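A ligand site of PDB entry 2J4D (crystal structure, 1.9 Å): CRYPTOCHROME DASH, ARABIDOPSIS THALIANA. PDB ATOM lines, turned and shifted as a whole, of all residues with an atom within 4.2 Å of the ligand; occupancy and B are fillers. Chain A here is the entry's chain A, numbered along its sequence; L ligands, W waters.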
ATOM      1  N   TYR A 272      19.153  12.731  14.523  1.00  0.00           N
ATOM      2  CA  TYR A 272      18.819  13.787  15.466  1.00  0.00           C
ATOM      3  C   TYR A 272      19.803  14.967  15.485  1.00  0.00           C
ATOM      4  O   TYR A 272      19.394  16.119  15.356  1.00  0.00           O
ATOM      5  CB  TYR A 272      18.706  13.203  16.884  1.00  0.00           C
ATOM      6  CG  TYR A 272      18.683  14.250  17.974  1.00  0.00           C
ATOM      7  CD1 TYR A 272      17.566  15.084  18.139  1.00  0.00           C
ATOM      8  CD2 TYR A 272      19.800  14.483  18.758  1.00  0.00           C
ATOM      9  CE1 TYR A 272      17.588  16.137  19.042  1.00  0.00           C
ATOM     10  CE2 TYR A 272      19.843  15.532  19.669  1.00  0.00           C
ATOM     11  CZ  TYR A 272      18.735  16.355  19.808  1.00  0.00           C
ATOM     12  OH  TYR A 272      18.787  17.454  20.638  1.00  0.00           O
ATOM     13  N   SER A 285      13.423  17.279  16.051  1.00  0.00           N
ATOM     14  CA  SER A 285      13.986  16.974  17.377  1.00  0.00           C
ATOM     15  C   SER A 285      13.070  16.036  18.135  1.00  0.00           C
ATOM     16  O   SER A 285      11.974  15.749  17.685  1.00  0.00           O
ATOM     17  CB  SER A 285      14.194  18.278  18.165  1.00  0.00           C
ATOM     18  OG  SER A 285      12.960  18.909  18.445  1.00  0.00           O
ATOM     19  N   THR A 286      13.508  15.547  19.304  1.00  0.00           N
ATOM     20  CA  THR A 286      12.678  14.607  20.043  1.00  0.00           C
ATOM     21  C   THR A 286      11.319  15.126  20.485  1.00  0.00           C
ATOM     22  O   THR A 286      10.363  14.349  20.542  1.00  0.00           O
ATOM     23  CB  THR A 286      13.376  14.078  21.328  1.00  0.00           C
ATOM     24  OG1 THR A 286      13.434  15.126  22.298  1.00  0.00           O
ATOM     25  CG2 THR A 286      14.781  13.549  21.019  1.00  0.00           C
ATOM     26  N   LYS A 287      11.241  16.416  20.786  1.00  0.00           N
ATOM     27  CA  LYS A 287      10.022  17.034  21.306  1.00  0.00           C
ATOM     28  C   LYS A 287       9.635  16.366  22.646  1.00  0.00           C
ATOM     29  O   LYS A 287       8.462  16.336  23.031  1.00  0.00           O
ATOM     30  CB  LYS A 287       8.875  16.905  20.300  1.00  0.00           C
ATOM     31  CG  LYS A 287       9.177  17.553  18.954  1.00  0.00           C
ATOM     32  CD  LYS A 287       9.549  19.025  19.102  1.00  0.00           C
ATOM     33  CE  LYS A 287       9.745  19.691  17.736  1.00  0.00           C
ATOM     34  NZ  LYS A 287      10.773  19.003  16.886  1.00  0.00           N
ATOM     35  N   PHE A 288      10.611  15.834  23.370  1.00  0.00           N
ATOM     36  CA  PHE A 288      10.307  15.186  24.651  1.00  0.00           C
ATOM     37  C   PHE A 288      10.087  16.172  25.805  1.00  0.00           C
ATOM     38  O   PHE A 288       9.514  15.808  26.838  1.00  0.00           O
ATOM     39  CB  PHE A 288      11.439  14.249  25.118  1.00  0.00           C
ATOM     40  CG  PHE A 288      11.717  13.081  24.209  1.00  0.00           C
ATOM     41  CD1 PHE A 288      10.783  12.633  23.275  1.00  0.00           C
ATOM     42  CD2 PHE A 288      12.931  12.383  24.323  1.00  0.00           C
ATOM     43  CE1 PHE A 288      11.053  11.516  22.479  1.00  0.00           C
ATOM     44  CE2 PHE A 288      13.205  11.276  23.546  1.00  0.00           C
ATOM     45  CZ  PHE A 288      12.262  10.834  22.611  1.00  0.00           C
ATOM     46  N   SER A 289      10.543  17.413  25.654  1.00  0.00           N
ATOM     47  CA  SER A 289      10.497  18.372  26.746  1.00  0.00           C
ATOM     48  C   SER A 289       9.237  18.551  27.592  1.00  0.00           C
ATOM     49  O   SER A 289       9.330  18.626  28.819  1.00  0.00           O
ATOM     50  CB  SER A 289      11.000  19.734  26.271  1.00  0.00           C
ATOM     51  OG  SER A 289      10.139  20.289  25.293  1.00  0.00           O
ATOM     52  N   LEU A 292       8.921  15.582  29.867  1.00  0.00           N
ATOM     53  CA  LEU A 292       9.997  15.549  30.859  1.00  0.00           C
ATOM     54  C   LEU A 292       9.701  16.569  31.954  1.00  0.00           C
ATOM     55  O   LEU A 292       9.894  16.298  33.141  1.00  0.00           O
ATOM     56  CB  LEU A 292      11.346  15.853  30.204  1.00  0.00           C
ATOM     57  CG  LEU A 292      11.964  14.666  29.451  1.00  0.00           C
ATOM     58  CD1 LEU A 292      13.096  15.134  28.558  1.00  0.00           C
ATOM     59  CD2 LEU A 292      12.452  13.638  30.473  1.00  0.00           C
ATOM     60  N   GLU A 325      22.228  16.327  25.248  1.00  0.00           N
ATOM     61  CA  GLU A 325      21.230  17.340  25.577  1.00  0.00           C
ATOM     62  C   GLU A 325      20.538  17.087  26.924  1.00  0.00           C
ATOM     63  O   GLU A 325      20.219  18.028  27.659  1.00  0.00           O
ATOM     64  CB  GLU A 325      20.189  17.449  24.456  1.00  0.00           C
ATOM     65  CG  GLU A 325      20.768  17.911  23.102  1.00  0.00           C
ATOM     66  CD  GLU A 325      21.487  19.264  23.153  1.00  0.00           C
ATOM     67  OE1 GLU A 325      21.174  20.101  24.023  1.00  0.00           O
ATOM     68  OE2 GLU A 325      22.377  19.490  22.299  1.00  0.00           O
ATOM     69  N   LEU A 326      20.323  15.814  27.260  1.00  0.00           N
ATOM     70  CA  LEU A 326      19.699  15.485  28.537  1.00  0.00           C
ATOM     71  C   LEU A 326      20.650  15.860  29.679  1.00  0.00           C
ATOM     72  O   LEU A 326      20.199  16.147  30.786  1.00  0.00           O
ATOM     73  CB  LEU A 326      19.351  13.991  28.616  1.00  0.00           C
ATOM     74  CG  LEU A 326      18.098  13.591  27.831  1.00  0.00           C
ATOM     75  CD1 LEU A 326      17.935  12.071  27.855  1.00  0.00           C
ATOM     76  CD2 LEU A 326      16.879  14.285  28.444  1.00  0.00           C
ATOM     77  N   TRP A 328      22.427  18.480  29.647  1.00  0.00           N
ATOM     78  CA  TRP A 328      22.248  19.914  29.810  1.00  0.00           C
ATOM     79  C   TRP A 328      21.086  20.123  30.776  1.00  0.00           C
ATOM     80  O   TRP A 328      21.117  21.029  31.614  1.00  0.00           O
ATOM     81  CB  TRP A 328      21.916  20.594  28.463  1.00  0.00           C
ATOM     82  CG  TRP A 328      23.106  21.216  27.787  1.00  0.00           C
ATOM     83  CD1 TRP A 328      23.768  20.756  26.682  1.00  0.00           C
ATOM     84  CD2 TRP A 328      23.787  22.410  28.183  1.00  0.00           C
ATOM     85  NE1 TRP A 328      24.815  21.591  26.364  1.00  0.00           N
ATOM     86  CE2 TRP A 328      24.846  22.621  27.271  1.00  0.00           C
ATOM     87  CE3 TRP A 328      23.604  23.333  29.220  1.00  0.00           C
ATOM     88  CZ2 TRP A 328      25.715  23.719  27.360  1.00  0.00           C
ATOM     89  CZ3 TRP A 328      24.469  24.426  29.317  1.00  0.00           C
ATOM     90  CH2 TRP A 328      25.509  24.605  28.389  1.00  0.00           C
ATOM     91  N   ARG A 329      20.058  19.289  30.662  1.00  0.00           N
ATOM     92  CA  ARG A 329      18.912  19.382  31.572  1.00  0.00           C
ATOM     93  C   ARG A 329      19.386  19.078  33.003  1.00  0.00           C
ATOM     94  O   ARG A 329      19.025  19.788  33.953  1.00  0.00           O
ATOM     95  CB  ARG A 329      17.824  18.389  31.148  1.00  0.00           C
ATOM     96  CG  ARG A 329      16.660  18.270  32.119  1.00  0.00           C
ATOM     97  CD  ARG A 329      15.511  17.472  31.519  1.00  0.00           C
ATOM     98  NE  ARG A 329      14.455  17.262  32.496  1.00  0.00           N
ATOM     99  CZ  ARG A 329      14.497  16.333  33.450  1.00  0.00           C
ATOM    100  NH1 ARG A 329      15.534  15.513  33.554  1.00  0.00           N
ATOM    101  NH2 ARG A 329      13.506  16.252  34.332  1.00  0.00           N
ATOM    102  N   PHE A 332      21.412  22.133  34.443  1.00  0.00           N
ATOM    103  CA  PHE A 332      20.657  23.263  34.965  1.00  0.00           C
ATOM    104  C   PHE A 332      19.891  22.918  36.234  1.00  0.00           C
ATOM    105  O   PHE A 332      19.688  23.772  37.096  1.00  0.00           O
ATOM    106  CB  PHE A 332      19.697  23.811  33.893  1.00  0.00           C
ATOM    107  CG  PHE A 332      20.391  24.703  32.878  1.00  0.00           C
ATOM    108  CD1 PHE A 332      21.098  25.830  33.288  1.00  0.00           C
ATOM    109  CD2 PHE A 332      20.346  24.399  31.524  1.00  0.00           C
ATOM    110  CE1 PHE A 332      21.738  26.645  32.366  1.00  0.00           C
ATOM    111  CE2 PHE A 332      20.987  25.211  30.588  1.00  0.00           C
ATOM    112  CZ  PHE A 332      21.689  26.333  31.006  1.00  0.00           C
ATOM    113  N   PHE A 388       5.089  25.950  22.604  1.00  0.00           N
ATOM    114  CA  PHE A 388       6.408  25.373  22.324  1.00  0.00           C
ATOM    115  C   PHE A 388       7.174  26.297  21.377  1.00  0.00           C
ATOM    116  O   PHE A 388       6.578  27.065  20.633  1.00  0.00           O
ATOM    117  CB  PHE A 388       6.255  23.986  21.683  1.00  0.00           C
ATOM    118  CG  PHE A 388       7.567  23.269  21.472  1.00  0.00           C
ATOM    119  CD1 PHE A 388       8.108  22.480  22.478  1.00  0.00           C
ATOM    120  CD2 PHE A 388       8.258  23.390  20.265  1.00  0.00           C
ATOM    121  CE1 PHE A 388       9.336  21.829  22.309  1.00  0.00           C
ATOM    122  CE2 PHE A 388       9.495  22.731  20.084  1.00  0.00           C
ATOM    123  CZ  PHE A 388      10.028  21.952  21.117  1.00  0.00           C
ATOM    124  N   MET A 389       8.501  26.207  21.437  1.00  0.00           N
ATOM    125  CA  MET A 389       9.383  26.973  20.552  1.00  0.00           C
ATOM    126  C   MET A 389      10.638  26.136  20.420  1.00  0.00           C
ATOM    127  O   MET A 389      11.067  25.516  21.398  1.00  0.00           O
ATOM    128  CB  MET A 389       9.730  28.346  21.136  1.00  0.00           C
ATOM    129  CG  MET A 389      10.501  29.232  20.147  1.00  0.00           C
ATOM    130  SD  MET A 389      11.092  30.808  20.822  1.00  0.00           S
ATOM    131  CE  MET A 389       9.538  31.542  21.419  1.00  0.00           C
ATOM    132  N   SER A 390      11.218  26.090  19.213  1.00  0.00           N
ATOM    133  CA  SER A 390      12.429  25.311  18.989  1.00  0.00           C
ATOM    134  C   SER A 390      13.555  25.898  19.837  1.00  0.00           C
ATOM    135  O   SER A 390      13.523  27.085  20.180  1.00  0.00           O
ATOM    136  CB  SER A 390      12.859  25.343  17.519  1.00  0.00           C
ATOM    137  OG  SER A 390      13.278  26.643  17.154  1.00  0.00           O
ATOM    138  N   ASN A 391      14.546  25.077  20.155  1.00  0.00           N
ATOM    139  CA  ASN A 391      15.684  25.541  20.940  1.00  0.00           C
ATOM    140  C   ASN A 391      16.383  26.706  20.219  1.00  0.00           C
ATOM    141  O   ASN A 391      16.777  27.686  20.836  1.00  0.00           O
ATOM    142  CB  ASN A 391      16.674  24.408  21.159  1.00  0.00           C
ATOM    143  CG  ASN A 391      17.915  24.854  21.913  1.00  0.00           C
ATOM    144  OD1 ASN A 391      17.819  25.365  23.031  1.00  0.00           O
ATOM    145  ND2 ASN A 391      19.072  24.681  21.293  1.00  0.00           N
ATOM    146  N   ARG A 394      14.321  29.867  20.668  1.00  0.00           N
ATOM    147  CA  ARG A 394      14.403  30.407  22.022  1.00  0.00           C
ATOM    148  C   ARG A 394      15.696  31.184  22.218  1.00  0.00           C
ATOM    149  O   ARG A 394      15.700  32.240  22.861  1.00  0.00           O
ATOM    150  CB  ARG A 394      14.316  29.288  23.066  1.00  0.00           C
ATOM    151  CG  ARG A 394      13.050  28.469  22.986  1.00  0.00           C
ATOM    152  CD  ARG A 394      12.946  27.460  24.147  1.00  0.00           C
ATOM    153  NE  ARG A 394      12.071  26.345  23.780  1.00  0.00           N
ATOM    154  CZ  ARG A 394      11.457  25.537  24.644  1.00  0.00           C
ATOM    155  NH1 ARG A 394      11.591  25.726  25.944  1.00  0.00           N
ATOM    156  NH2 ARG A 394      10.704  24.530  24.188  1.00  0.00           N
ATOM    157  N   GLN A 395      16.804  30.670  21.697  1.00  0.00           N
ATOM    158  CA  GLN A 395      18.066  31.373  21.849  1.00  0.00           C
ATOM    159  C   GLN A 395      18.012  32.713  21.105  1.00  0.00           C
ATOM    160  O   GLN A 395      18.493  33.740  21.593  1.00  0.00           O
ATOM    161  CB  GLN A 395      19.225  30.529  21.284  1.00  0.00           C
ATOM    162  CG  GLN A 395      19.420  29.187  21.975  1.00  0.00           C
ATOM    163  CD  GLN A 395      20.649  28.479  21.472  1.00  0.00           C
ATOM    164  OE1 GLN A 395      21.774  28.869  21.781  1.00  0.00           O
ATOM    165  NE2 GLN A 395      20.452  27.427  20.680  1.00  0.00           N
ATOM    166  N   CYS A 398      15.590  35.312  22.701  1.00  0.00           N
ATOM    167  CA  CYS A 398      16.182  35.743  23.974  1.00  0.00           C
ATOM    168  C   CYS A 398      17.219  36.844  23.700  1.00  0.00           C
ATOM    169  O   CYS A 398      17.231  37.895  24.343  1.00  0.00           O
ATOM    170  CB  CYS A 398      16.856  34.557  24.677  1.00  0.00           C
ATOM    171  SG  CYS A 398      17.992  35.053  26.010  1.00  0.00           S
ATOM    172  N   PHE A 416       7.986  33.280  29.076  1.00  0.00           N
ATOM    173  CA  PHE A 416       8.227  31.890  28.704  1.00  0.00           C
ATOM    174  C   PHE A 416       7.591  31.036  29.821  1.00  0.00           C
ATOM    175  O   PHE A 416       6.982  29.995  29.549  1.00  0.00           O
ATOM    176  CB  PHE A 416       9.737  31.604  28.612  1.00  0.00           C
ATOM    177  CG  PHE A 416      10.314  31.749  27.231  1.00  0.00           C
ATOM    178  CD1 PHE A 416       9.864  32.742  26.362  1.00  0.00           C
ATOM    179  CD2 PHE A 416      11.371  30.932  26.817  1.00  0.00           C
ATOM    180  CE1 PHE A 416      10.438  32.908  25.093  1.00  0.00           C
ATOM    181  CE2 PHE A 416      11.961  31.089  25.564  1.00  0.00           C
ATOM    182  CZ  PHE A 416      11.494  32.076  24.695  1.00  0.00           C
ATOM    183  N   LEU A 420       5.258  28.289  28.012  1.00  0.00           N
ATOM    184  CA  LEU A 420       5.838  26.975  27.736  1.00  0.00           C
ATOM    185  C   LEU A 420       5.216  25.739  28.357  1.00  0.00           C
ATOM    186  O   LEU A 420       5.083  25.654  29.564  1.00  0.00           O
ATOM    187  CB  LEU A 420       7.321  26.968  28.101  1.00  0.00           C
ATOM    188  CG  LEU A 420       8.245  27.821  27.236  1.00  0.00           C
ATOM    189  CD1 LEU A 420       9.622  27.883  27.873  1.00  0.00           C
ATOM    190  CD2 LEU A 420       8.316  27.227  25.832  1.00  0.00           C
ATOM    191  N   ASP A 422       6.683  23.014  28.393  1.00  0.00           N
ATOM    192  CA  ASP A 422       7.809  22.408  29.092  1.00  0.00           C
ATOM    193  C   ASP A 422       8.451  23.295  30.129  1.00  0.00           C
ATOM    194  O   ASP A 422       9.573  23.023  30.570  1.00  0.00           O
ATOM    195  CB  ASP A 422       8.885  21.940  28.101  1.00  0.00           C
ATOM    196  CG  ASP A 422       9.450  23.068  27.225  1.00  0.00           C
ATOM    197  OD1 ASP A 422       9.546  24.222  27.693  1.00  0.00           O
ATOM    198  OD2 ASP A 422       9.813  22.781  26.058  1.00  0.00           O
ATOM    199  N   TYR A 423       7.754  24.343  30.560  1.00  0.00           N
ATOM    200  CA  TYR A 423       8.340  25.241  31.536  1.00  0.00           C
ATOM    201  C   TYR A 423       8.894  24.475  32.725  1.00  0.00           C
ATOM    202  O   TYR A 423       8.207  23.665  33.335  1.00  0.00           O
ATOM    203  CB  TYR A 423       7.335  26.250  32.060  1.00  0.00           C
ATOM    204  CG  TYR A 423       7.886  26.986  33.267  1.00  0.00           C
ATOM    205  CD1 TYR A 423       8.986  27.833  33.136  1.00  0.00           C
ATOM    206  CD2 TYR A 423       7.337  26.803  34.540  1.00  0.00           C
ATOM    207  CE1 TYR A 423       9.541  28.480  34.244  1.00  0.00           C
ATOM    208  CE2 TYR A 423       7.888  27.445  35.656  1.00  0.00           C
ATOM    209  CZ  TYR A 423       8.985  28.280  35.491  1.00  0.00           C
ATOM    210  OH  TYR A 423       9.532  28.929  36.585  1.00  0.00           O
ATOM    211  N   ASP A 424      10.159  24.785  33.038  1.00  0.00           N
ATOM    212  CA  ASP A 424      10.891  24.193  34.142  1.00  0.00           C
ATOM    213  C   ASP A 424      11.704  25.364  34.683  1.00  0.00           C
ATOM    214  O   ASP A 424      12.454  26.001  33.934  1.00  0.00           O
ATOM    215  CB  ASP A 424      11.809  23.084  33.591  1.00  0.00           C
ATOM    216  CG  ASP A 424      12.633  22.422  34.667  1.00  0.00           C
ATOM    217  OD1 ASP A 424      12.428  21.213  34.905  1.00  0.00           O
ATOM    218  OD2 ASP A 424      13.485  23.106  35.273  1.00  0.00           O
ATOM    219  N   SER A 427      15.629  24.915  33.972  1.00  0.00           N
ATOM    220  CA  SER A 427      15.978  25.039  32.561  1.00  0.00           C
ATOM    221  C   SER A 427      15.617  26.393  31.978  1.00  0.00           C
ATOM    222  O   SER A 427      16.388  26.971  31.220  1.00  0.00           O
ATOM    223  CB  SER A 427      15.301  23.937  31.751  1.00  0.00           C
ATOM    224  OG  SER A 427      15.880  22.670  32.006  1.00  0.00           O
ATOM    225  N   ASN A 428      14.440  26.925  32.322  1.00  0.00           N
ATOM    226  CA  ASN A 428      14.027  28.206  31.759  1.00  0.00           C
ATOM    227  C   ASN A 428      14.920  29.347  32.200  1.00  0.00           C
ATOM    228  O   ASN A 428      15.531  30.037  31.394  1.00  0.00           O
ATOM    229  CB  ASN A 428      12.583  28.527  32.120  1.00  0.00           C
ATOM    230  CG  ASN A 428      12.053  29.735  31.367  1.00  0.00           C
ATOM    231  OD1 ASN A 428      12.065  29.743  30.141  1.00  0.00           O
ATOM    232  ND2 ASN A 428      11.590  30.748  32.091  1.00  0.00           N
ATOM    233  N   ASN A 431      18.670  28.765  31.171  1.00  0.00           N
ATOM    234  CA  ASN A 431      18.981  29.152  29.810  1.00  0.00           C
ATOM    235  C   ASN A 431      18.850  30.662  29.600  1.00  0.00           C
ATOM    236  O   ASN A 431      19.626  31.243  28.834  1.00  0.00           O
ATOM    237  CB  ASN A 431      18.086  28.389  28.822  1.00  0.00           C
ATOM    238  CG  ASN A 431      18.607  26.999  28.523  1.00  0.00           C
ATOM    239  OD1 ASN A 431      19.559  26.831  27.760  1.00  0.00           O
ATOM    240  ND2 ASN A 431      17.982  25.986  29.116  1.00  0.00           N
ATOM    241  N   TRP A 432      17.893  31.303  30.260  1.00  0.00           N
ATOM    242  CA  TRP A 432      17.744  32.750  30.118  1.00  0.00           C
ATOM    243  C   TRP A 432      18.960  33.496  30.686  1.00  0.00           C
ATOM    244  O   TRP A 432      19.432  34.455  30.071  1.00  0.00           O
ATOM    245  CB  TRP A 432      16.466  33.277  30.784  1.00  0.00           C
ATOM    246  CG  TRP A 432      15.278  33.286  29.858  1.00  0.00           C
ATOM    247  CD1 TRP A 432      14.335  32.301  29.717  1.00  0.00           C
ATOM    248  CD2 TRP A 432      14.949  34.292  28.896  1.00  0.00           C
ATOM    249  NE1 TRP A 432      13.441  32.640  28.715  1.00  0.00           N
ATOM    250  CE2 TRP A 432      13.800  33.851  28.193  1.00  0.00           C
ATOM    251  CE3 TRP A 432      15.516  35.526  28.547  1.00  0.00           C
ATOM    252  CZ2 TRP A 432      13.215  34.607  27.170  1.00  0.00           C
ATOM    253  CZ3 TRP A 432      14.934  36.273  27.534  1.00  0.00           C
ATOM    254  CH2 TRP A 432      13.794  35.811  26.850  1.00  0.00           C
HETATM  255  P1  LIG L   1      15.875  18.156  22.026  1.00  0.00           P
HETATM  256  O1  LIG L   1      15.186  16.982  21.460  1.00  0.00           O
HETATM  257  O2  LIG L   1      16.886  18.881  21.225  1.00  0.00           O
HETATM  258  O3  LIG L   1      16.577  17.764  23.415  1.00  0.00           O
HETATM  259  C1  LIG L   1      16.155  16.581  24.146  1.00  0.00           C
HETATM  260  C2  LIG L   1      15.947  16.986  25.612  1.00  0.00           C
HETATM  261  O4  LIG L   1      17.168  17.509  26.121  1.00  0.00           O
HETATM  262  C3  LIG L   1      14.902  18.068  25.840  1.00  0.00           C
HETATM  263  O5  LIG L   1      13.575  17.571  25.820  1.00  0.00           O
HETATM  264  C4  LIG L   1      15.352  18.623  27.158  1.00  0.00           C
HETATM  265  O6  LIG L   1      14.834  17.969  28.297  1.00  0.00           O
HETATM  266  C5  LIG L   1      16.895  18.565  27.058  1.00  0.00           C
HETATM  267  N1  LIG L   1      17.546  19.805  26.582  1.00  0.00           N
HETATM  268  C6  LIG L   1      17.947  20.108  25.297  1.00  0.00           C
HETATM  269  N2  LIG L   1      18.508  21.304  25.215  1.00  0.00           N
HETATM  270  C7  LIG L   1      18.474  21.799  26.495  1.00  0.00           C
HETATM  271  C8  LIG L   1      18.914  23.032  27.051  1.00  0.00           C
HETATM  272  N3  LIG L   1      19.517  23.992  26.367  1.00  0.00           N
HETATM  273  N4  LIG L   1      18.716  23.211  28.408  1.00  0.00           N
HETATM  274  C9  LIG L   1      18.098  22.246  29.158  1.00  0.00           C
HETATM  275  N5  LIG L   1      17.660  21.053  28.688  1.00  0.00           N
HETATM  276  C10 LIG L   1      17.857  20.879  27.358  1.00  0.00           C
HETATM  277  N6  LIG L   1      13.813  23.526  28.262  1.00  0.00           N
HETATM  278  C11 LIG L   1      12.893  23.034  29.166  1.00  0.00           C
HETATM  279  O7  LIG L   1      12.770  21.846  29.359  1.00  0.00           O
HETATM  280  N7  LIG L   1      12.097  23.962  29.869  1.00  0.00           N
HETATM  281  C12 LIG L   1      12.171  25.336  29.704  1.00  0.00           C
HETATM  282  O8  LIG L   1      11.432  26.104  30.360  1.00  0.00           O
HETATM  283  C13 LIG L   1      13.120  25.831  28.779  1.00  0.00           C
HETATM  284  N8  LIG L   1      13.269  27.211  28.543  1.00  0.00           N
HETATM  285  C14 LIG L   1      14.281  27.694  27.708  1.00  0.00           C
HETATM  286  C15 LIG L   1      14.497  29.072  27.583  1.00  0.00           C
HETATM  287  C16 LIG L   1      15.512  29.596  26.747  1.00  0.00           C
HETATM  288  C17 LIG L   1      15.705  31.090  26.650  1.00  0.00           C
HETATM  289  C18 LIG L   1      16.341  28.674  26.015  1.00  0.00           C
HETATM  290  C19 LIG L   1      17.454  29.141  25.085  1.00  0.00           C
HETATM  291  C20 LIG L   1      16.130  27.284  26.136  1.00  0.00           C
HETATM  292  C21 LIG L   1      15.106  26.768  26.984  1.00  0.00           C
HETATM  293  N9  LIG L   1      14.869  25.363  27.122  1.00  0.00           N
HETATM  294  C22 LIG L   1      13.920  24.890  28.071  1.00  0.00           C
HETATM  295  C23 LIG L   1      15.858  24.382  26.592  1.00  0.00           C
HETATM  296  C24 LIG L   1      15.595  23.827  25.171  1.00  0.00           C
HETATM  297  O9  LIG L   1      15.381  24.895  24.279  1.00  0.00           O
HETATM  298  C25 LIG L   1      14.381  22.910  25.190  1.00  0.00           C
HETATM  299  O10 LIG L   1      14.552  21.848  26.152  1.00  0.00           O
HETATM  300  C26 LIG L   1      14.077  22.206  23.854  1.00  0.00           C
HETATM  301  O11 LIG L   1      13.797  23.185  22.840  1.00  0.00           O
HETATM  302  C27 LIG L   1      12.875  21.290  24.032  1.00  0.00           C
HETATM  303  O12 LIG L   1      12.597  20.612  22.799  1.00  0.00           O
HETATM  304  P2  LIG L   1      13.108  19.170  22.416  1.00  0.00           P
HETATM  305  O13 LIG L   1      12.545  18.275  23.435  1.00  0.00           O
HETATM  306  O14 LIG L   1      12.672  18.871  21.021  1.00  0.00           O
HETATM  307  O15 LIG L   1      14.694  19.202  22.351  1.00  0.00           O
HETATM  308  O   HOH W   1      13.864  22.344  20.071  1.00  0.00           O
HETATM  309  O   HOH W   2      20.127  26.328  24.234  1.00  0.00           O
HETATM  310  O   HOH W   3      18.542  20.928  22.083  1.00  0.00           O
HETATM  311  O   HOH W   4      20.980  22.971  23.921  1.00  0.00           O
HETATM  312  O   HOH W   5      11.988  19.272  29.753  1.00  0.00           O
HETATM  313  O   HOH W   6      16.180  20.913  19.374  1.00  0.00           O
HETATM  314  O   HOH W   7      15.200  20.849  30.289  1.00  0.00           O
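Water W5 lies within hydrogen-bond range of O7 of the ligand (2.7 Å) and O of Ser 289 (2.9 Å). Water W3 lies within hydrogen-bond range of O2 of the ligand (2.8 Å) and OE1 of Glu 325 (3.4 Å). Water W7 bridges OG of Ser 427 and O7 of the ligand. Water W1 lies within hydrogen-bond range of N of Asn 391 and O11 of the ligand. Water W4 lies within hydrogen-bond range of OE1 of Glu 325 and N3 of the ligand. Water W2 bridges the side-chain amide oxygen (OD1) of Asn 391 (2.8 Å) and a nitrogen (N3) of the ligand (3.2 Å).
The side-chain hydroxyl of Tyr 272 is in hydrogen-bond range of an oxygen (O2) of the ligand, 2.4 Å away. The side-chain hydroxyl (OG) of Ser 285 lies within hydrogen-bond range of an oxygen (O14) of the ligand (2.6 Å). N of Thr 286 lies within hydrogen-bond range of O1 of the ligand (3.1 Å). An oxygen (O1) of the ligand lies within hydrogen-bond range of the side-chain hydroxyl (OG1) of Thr 286 (2.7 Å). N of Asn 391 is in hydrogen-bond range of O11 of the ligand, at 3.4 Å. O9 of the ligand lies within hydrogen-bond range of OD1 of Asn 391 (2.8 Å). O of Asp 422 is in hydrogen-bond range of N7 of the ligand (2.8 Å). N7 of the ligand lies within hydrogen-bond range of OD1 of Asp 422. The backbone NH of Lys 287 is in hydrogen-bond range of an oxygen (O14) of the ligand (2.9 Å). ND2 of Asn 431 lies within hydrogen-bond range of N4 of the ligand (3.0 Å). An oxygen (O5) of the ligand sits at hydrogen-bond distance from the backbone NH (N) of Ser 289. An oxygen (O13) of the ligand sits at hydrogen-bond distance from the backbone NH (N) of Phe 288 (3.1 Å). The side-chain amide oxygen of Asn 428 lies close to a nitrogen (N8) of the ligand (3.2 Å). NH1 of Arg 394 lies close to N8 of the ligand (3.4 Å). N of Asp 424 is in hydrogen-bond range of O8 of the ligand, at 3.2 Å.
The side-chain amino group (NZ) of Lys 287 is in hydrogen-bond range of the side-chain hydroxyl (OG) of Ser 285, at 2.7 Å. N of Phe 288 sits close to OG1 of Thr 286, at 3.1 Å. The side-chain amide nitrogen (ND2) of Asn 391 sits close to the side-chain amide nitrogen (NE2) of Gln 395 (3.1 Å). The side-chain carboxylate of Asp 422 lies within hydrogen-bond range of the side-chain hydroxyl of Ser 289, 2.6 Å away. The side-chain carboxylate (OD2) of Asp 422 lies within salt-bridge range of the guanidinium group (NH2) of Arg 394 (2.7 Å). O of Ser 427 lies within hydrogen-bond range of ND2 of Asn 431 (2.8 Å). The guanidinium group of Arg 394 is in hydrogen-bond range of the backbone carbonyl oxygen of Met 389 (2.7 Å). The side-chain carboxylate of Asp 424 sits at hydrogen-bond distance from the backbone NH of Ser 427 (3.1 Å).
OE1 of Glu 325 sits close to N2 of the ligand (3.2 Å). Residues that only touch the ligand: Leu 292 (3.3 Å), Leu 326 (3.8 Å), Arg 329 (3.3 Å), Phe 332 (3.7 Å), Phe 388 (3.4 Å), Met 389 (3.9 Å), Gln 395 (3.7 Å), Phe 416 (3.7 Å), Leu 420 (3.6 Å), Tyr 423 (3.4 Å), Ser 427 (3.6 Å) and Trp 432 (3.4 Å). 25 residues have an atom within 4 Å of the ligand: Tyr 272, Ser 285, Thr 286, Lys 287, Phe 288, Ser 289, Leu 292, Glu 325, Leu 326, Arg 329, Phe 332, Phe 388, Met 389, Asn 391, Arg 394, Gln 395, Phe 416, Leu 420, Asp 422, Tyr 423, Asp 424, Ser 427, Asn 428, Asn 431 and Trp 432.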
